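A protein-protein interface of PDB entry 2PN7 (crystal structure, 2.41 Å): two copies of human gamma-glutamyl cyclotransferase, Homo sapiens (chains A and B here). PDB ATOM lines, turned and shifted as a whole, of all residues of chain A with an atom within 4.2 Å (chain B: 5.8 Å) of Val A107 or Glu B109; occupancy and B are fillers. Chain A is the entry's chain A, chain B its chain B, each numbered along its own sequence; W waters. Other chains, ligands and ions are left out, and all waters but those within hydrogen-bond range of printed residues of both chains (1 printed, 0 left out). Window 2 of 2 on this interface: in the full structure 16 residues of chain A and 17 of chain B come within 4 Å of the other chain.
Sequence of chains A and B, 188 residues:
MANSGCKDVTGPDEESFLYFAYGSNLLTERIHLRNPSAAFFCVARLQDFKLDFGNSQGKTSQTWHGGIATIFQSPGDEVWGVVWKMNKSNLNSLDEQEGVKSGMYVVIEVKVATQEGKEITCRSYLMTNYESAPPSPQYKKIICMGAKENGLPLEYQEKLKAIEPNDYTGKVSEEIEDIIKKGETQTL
OE2 of Glu B109 lies within salt-bridge range of NH2 of Arg A123 (2.8 Å). The backbone NH (N) of Glu B109 is in hydrogen-bond range of the backbone carbonyl oxygen (O) of Val A107 (3.1 Å).
The side-chain hydroxyl (OH) of Tyr A125 lies within hydrogen-bond range of the guanidinium group (NE) of Arg A123 (3.5 Å). The backbone NH (N) of Ile A108 is in hydrogen-bond range of the backbone carbonyl oxygen (O) of Ser A124 (3.1 Å). OD1 of Asp A95 lies within salt-bridge range of NH2 of Arg A123. The backbone carbonyl oxygen of Ile B108 is in hydrogen-bond range of the backbone NH of Ser B124.
Among the printed residues, merely in contact across the chains: Val A107 with Ile B108 and Ile A108 with Val B107.
Val A107 touches two residues of chain B. Of the printed residues of chain B, Arg A123 touches Glu B109 (2.8 Å). Of the printed residues of chain A, Val B107 touches Ile A108. Of the printed residues of chain A, Ile B108 touches Val A107.
Printed residues of chain B that touch a printed residue of chain A: Val B107, Ile B108 and Glu B109. Hydrophobic or aromatic side chains of chain B that line the printed part of chain A: Ile B108. Among the printed residues, 4 pairs touch across the chains. Among the printed residues, Asp or Glu carboxylates within 4 Å of a Lys or Arg side-chain nitrogen of the other chain: Arg A123 with Glu B109 (2.8 Å).
Val A107 touches Ile B108, and with the chains exchanged Ile A108 touches Val B107.
Water W1 lies within hydrogen-bond range of O of Glu B109 (2.6 Å) and N of Val A107 (2.7 Å).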
ATOM      1  N   ASP A  95      -3.553 -31.994 -32.229  1.00  0.00           N
ATOM      2  CA  ASP A  95      -2.664 -30.914 -32.653  1.00  0.00           C
ATOM      3  C   ASP A  95      -2.759 -30.660 -34.149  1.00  0.00           C
ATOM      4  O   ASP A  95      -2.980 -29.523 -34.541  1.00  0.00           O
ATOM      5  CB  ASP A  95      -1.220 -31.189 -32.262  1.00  0.00           C
ATOM      6  CG  ASP A  95      -1.004 -31.145 -30.760  1.00  0.00           C
ATOM      7  OD1 ASP A  95      -1.964 -30.770 -30.044  1.00  0.00           O
ATOM      8  OD2 ASP A  95       0.122 -31.492 -30.309  1.00  0.00           O
ATOM      9  N   VAL A 100      -1.749 -26.582 -35.069  1.00  0.00           N
ATOM     10  CA  VAL A 100      -0.654 -26.098 -34.231  1.00  0.00           C
ATOM     11  C   VAL A 100       0.602 -25.759 -35.071  1.00  0.00           C
ATOM     12  O   VAL A 100       1.079 -24.613 -35.048  1.00  0.00           O
ATOM     13  CB  VAL A 100      -0.340 -27.086 -33.067  1.00  0.00           C
ATOM     14  CG1 VAL A 100       0.988 -26.739 -32.418  1.00  0.00           C
ATOM     15  CG2 VAL A 100      -1.425 -27.036 -32.048  1.00  0.00           C
ATOM     16  N   VAL A 106      -2.351 -22.407 -30.533  1.00  0.00           N
ATOM     17  CA  VAL A 106      -1.280 -22.829 -29.650  1.00  0.00           C
ATOM     18  C   VAL A 106      -1.898 -23.784 -28.624  1.00  0.00           C
ATOM     19  O   VAL A 106      -3.050 -23.615 -28.244  1.00  0.00           O
ATOM     20  CB  VAL A 106      -0.558 -21.607 -29.011  1.00  0.00           C
ATOM     21  CG1 VAL A 106      -1.425 -20.954 -27.976  1.00  0.00           C
ATOM     22  CG2 VAL A 106       0.792 -22.010 -28.414  1.00  0.00           C
ATOM     23  N   VAL A 107      -1.176 -24.826 -28.226  1.00  0.00           N
ATOM     24  CA  VAL A 107      -1.653 -25.685 -27.106  1.00  0.00           C
ATOM     25  C   VAL A 107      -1.601 -24.930 -25.765  1.00  0.00           C
ATOM     26  O   VAL A 107      -0.582 -24.324 -25.416  1.00  0.00           O
ATOM     27  CB  VAL A 107      -0.828 -26.992 -26.978  1.00  0.00           C
ATOM     28  CG1 VAL A 107      -1.336 -27.834 -25.811  1.00  0.00           C
ATOM     29  CG2 VAL A 107      -0.817 -27.767 -28.287  1.00  0.00           C
ATOM     30  N   ILE A 108      -2.712 -24.939 -25.044  1.00  0.00           N
ATOM     31  CA  ILE A 108      -2.776 -24.434 -23.673  1.00  0.00           C
ATOM     32  C   ILE A 108      -3.129 -25.502 -22.577  1.00  0.00           C
ATOM     33  O   ILE A 108      -3.621 -26.598 -22.879  1.00  0.00           O
ATOM     34  CB  ILE A 108      -3.733 -23.205 -23.564  1.00  0.00           C
ATOM     35  CG1 ILE A 108      -5.205 -23.583 -23.846  1.00  0.00           C
ATOM     36  CG2 ILE A 108      -3.241 -22.077 -24.436  1.00  0.00           C
ATOM     37  CD1 ILE A 108      -6.182 -22.401 -23.698  1.00  0.00           C
ATOM     38  N   ARG A 123      -6.435 -29.924 -21.513  1.00  0.00           N
ATOM     39  CA  ARG A 123      -5.797 -29.356 -22.680  1.00  0.00           C
ATOM     40  C   ARG A 123      -6.870 -28.562 -23.407  1.00  0.00           C
ATOM     41  O   ARG A 123      -8.047 -28.916 -23.354  1.00  0.00           O
ATOM     42  CB  ARG A 123      -5.288 -30.475 -23.563  1.00  0.00           C
ATOM     43  CG  ARG A 123      -4.358 -30.095 -24.674  1.00  0.00           C
ATOM     44  CD  ARG A 123      -3.903 -31.391 -25.277  1.00  0.00           C
ATOM     45  NE  ARG A 123      -2.916 -31.279 -26.349  1.00  0.00           N
ATOM     46  CZ  ARG A 123      -1.601 -31.344 -26.194  1.00  0.00           C
ATOM     47  NH1 ARG A 123      -1.054 -31.461 -24.980  1.00  0.00           N
ATOM     48  NH2 ARG A 123      -0.819 -31.272 -27.268  1.00  0.00           N
ATOM     49  N   SER A 124      -6.458 -27.461 -24.034  1.00  0.00           N
ATOM     50  CA  SER A 124      -7.274 -26.707 -24.956  1.00  0.00           C
ATOM     51  C   SER A 124      -6.376 -26.005 -26.003  1.00  0.00           C
ATOM     52  O   SER A 124      -5.197 -26.343 -26.163  1.00  0.00           O
ATOM     53  CB  SER A 124      -8.173 -25.698 -24.219  1.00  0.00           C
ATOM     54  OG  SER A 124      -9.293 -25.366 -25.047  1.00  0.00           O
ATOM     55  N   TYR A 125      -6.952 -25.044 -26.715  1.00  0.00           N
ATOM     56  CA  TYR A 125      -6.265 -24.301 -27.752  1.00  0.00           C
ATOM     57  C   TYR A 125      -6.805 -22.892 -27.800  1.00  0.00           C
ATOM     58  O   TYR A 125      -7.979 -22.633 -27.467  1.00  0.00           O
ATOM     59  CB  TYR A 125      -6.501 -24.952 -29.105  1.00  0.00           C
ATOM     60  CG  TYR A 125      -6.011 -26.369 -29.148  1.00  0.00           C
ATOM     61  CD1 TYR A 125      -4.751 -26.660 -29.636  1.00  0.00           C
ATOM     62  CD2 TYR A 125      -6.811 -27.423 -28.704  1.00  0.00           C
ATOM     63  CE1 TYR A 125      -4.277 -27.954 -29.657  1.00  0.00           C
ATOM     64  CE2 TYR A 125      -6.343 -28.749 -28.744  1.00  0.00           C
ATOM     65  CZ  TYR A 125      -5.076 -28.991 -29.217  1.00  0.00           C
ATOM     66  OH  TYR A 125      -4.580 -30.264 -29.246  1.00  0.00           O
ATOM     67  N   VAL B 107      -0.744 -20.727 -19.497  1.00  0.00           N
ATOM     68  CA  VAL B 107       0.167 -21.863 -19.676  1.00  0.00           C
ATOM     69  C   VAL B 107       0.007 -22.415 -21.086  1.00  0.00           C
ATOM     70  O   VAL B 107      -1.107 -22.674 -21.529  1.00  0.00           O
ATOM     71  CB  VAL B 107      -0.169 -23.087 -18.733  1.00  0.00           C
ATOM     72  CG1 VAL B 107       0.694 -24.295 -19.067  1.00  0.00           C
ATOM     73  CG2 VAL B 107      -0.047 -22.760 -17.239  1.00  0.00           C
ATOM     74  N   ILE B 108       1.138 -22.601 -21.773  1.00  0.00           N
ATOM     75  CA  ILE B 108       1.204 -23.301 -23.064  1.00  0.00           C
ATOM     76  C   ILE B 108       2.129 -24.559 -23.047  1.00  0.00           C
ATOM     77  O   ILE B 108       2.952 -24.751 -22.144  1.00  0.00           O
ATOM     78  CB  ILE B 108       1.657 -22.326 -24.197  1.00  0.00           C
ATOM     79  CG1 ILE B 108       3.104 -21.882 -23.964  1.00  0.00           C
ATOM     80  CG2 ILE B 108       0.691 -21.146 -24.302  1.00  0.00           C
ATOM     81  CD1 ILE B 108       3.663 -20.973 -24.999  1.00  0.00           C
ATOM     82  N   GLU B 109       1.952 -25.413 -24.045  1.00  0.00           N
ATOM     83  CA  GLU B 109       2.871 -26.491 -24.372  1.00  0.00           C
ATOM     84  C   GLU B 109       3.488 -26.090 -25.700  1.00  0.00           C
ATOM     85  O   GLU B 109       2.780 -25.777 -26.663  1.00  0.00           O
ATOM     86  CB  GLU B 109       2.106 -27.819 -24.502  1.00  0.00           C
ATOM     87  CG  GLU B 109       2.941 -29.061 -24.876  1.00  0.00           C
ATOM     88  CD  GLU B 109       2.136 -30.391 -24.789  1.00  0.00           C
ATOM     89  OE1 GLU B 109       2.022 -30.983 -23.670  1.00  0.00           O
ATOM     90  OE2 GLU B 109       1.608 -30.846 -25.843  1.00  0.00           O
ATOM     91  N   VAL B 110       4.810 -26.048 -25.747  1.00  0.00           N
ATOM     92  CA  VAL B 110       5.508 -25.832 -27.021  1.00  0.00           C
ATOM     93  C   VAL B 110       6.489 -26.951 -27.288  1.00  0.00           C
ATOM     94  O   VAL B 110       6.949 -27.642 -26.364  1.00  0.00           O
ATOM     95  CB  VAL B 110       6.314 -24.554 -27.047  1.00  0.00           C
ATOM     96  CG1 VAL B 110       5.400 -23.310 -27.256  1.00  0.00           C
ATOM     97  CG2 VAL B 110       7.211 -24.453 -25.817  1.00  0.00           C
ATOM     98  N   LYS B 111       6.807 -27.108 -28.569  1.00  0.00           N
ATOM     99  CA  LYS B 111       7.807 -28.044 -28.993  1.00  0.00           C
ATOM    100  C   LYS B 111       8.957 -27.241 -29.523  1.00  0.00           C
ATOM    101  O   LYS B 111       8.811 -26.541 -30.509  1.00  0.00           O
ATOM    102  CB  LYS B 111       7.258 -28.976 -30.066  1.00  0.00           C
ATOM    103  CG  LYS B 111       6.382 -30.090 -29.530  1.00  0.00           C
ATOM    104  CD  LYS B 111       6.010 -31.019 -30.670  1.00  0.00           C
ATOM    105  CE  LYS B 111       4.698 -31.733 -30.438  1.00  0.00           C
ATOM    106  NZ  LYS B 111       4.764 -32.693 -29.326  1.00  0.00           N
ATOM    107  N   THR B 121       9.624 -31.243 -25.716  1.00  0.00           N
ATOM    108  CA  THR B 121       8.265 -30.772 -25.392  1.00  0.00           C
ATOM    109  C   THR B 121       8.322 -30.104 -24.020  1.00  0.00           C
ATOM    110  O   THR B 121       8.682 -30.764 -23.031  1.00  0.00           O
ATOM    111  CB  THR B 121       7.184 -31.933 -25.433  1.00  0.00           C
ATOM    112  OG1 THR B 121       6.946 -32.351 -26.792  1.00  0.00           O
ATOM    113  CG2 THR B 121       5.832 -31.498 -24.792  1.00  0.00           C
ATOM    114  N   CYS B 122       7.965 -28.815 -23.971  1.00  0.00           N
ATOM    115  CA  CYS B 122       8.035 -28.029 -22.743  1.00  0.00           C
ATOM    116  C   CYS B 122       6.754 -27.270 -22.402  1.00  0.00           C
ATOM    117  O   CYS B 122       5.921 -27.035 -23.246  1.00  0.00           O
ATOM    118  CB  CYS B 122       9.130 -26.963 -22.809  1.00  0.00           C
ATOM    119  SG  CYS B 122      10.611 -27.347 -23.622  1.00  0.00           S
ATOM    120  N   ARG B 123       6.676 -26.846 -21.149  1.00  0.00           N
ATOM    121  CA  ARG B 123       5.712 -25.901 -20.666  1.00  0.00           C
ATOM    122  C   ARG B 123       6.305 -24.497 -20.883  1.00  0.00           C
ATOM    123  O   ARG B 123       7.492 -24.300 -20.727  1.00  0.00           O
ATOM    124  CB  ARG B 123       5.480 -26.182 -19.171  1.00  0.00           C
ATOM    125  CG  ARG B 123       4.403 -25.394 -18.456  1.00  0.00           C
ATOM    126  CD  ARG B 123       4.423 -25.671 -16.932  1.00  0.00           C
ATOM    127  NE  ARG B 123       3.170 -25.325 -16.231  1.00  0.00           N
ATOM    128  CZ  ARG B 123       2.054 -26.073 -16.215  1.00  0.00           C
ATOM    129  NH1 ARG B 123       1.983 -27.239 -16.867  1.00  0.00           N
ATOM    130  NH2 ARG B 123       0.989 -25.655 -15.529  1.00  0.00           N
ATOM    131  N   SER B 124       5.477 -23.525 -21.259  1.00  0.00           N
ATOM    132  CA  SER B 124       5.908 -22.125 -21.261  1.00  0.00           C
ATOM    133  C   SER B 124       4.676 -21.295 -20.987  1.00  0.00           C
ATOM    134  O   SER B 124       3.702 -21.815 -20.495  1.00  0.00           O
ATOM    135  CB  SER B 124       6.578 -21.736 -22.602  1.00  0.00           C
ATOM    136  OG  SER B 124       7.117 -20.427 -22.537  1.00  0.00           O
HETATM  137  O   HOH W   1       1.396 -25.462 -28.876  1.00  0.00           O
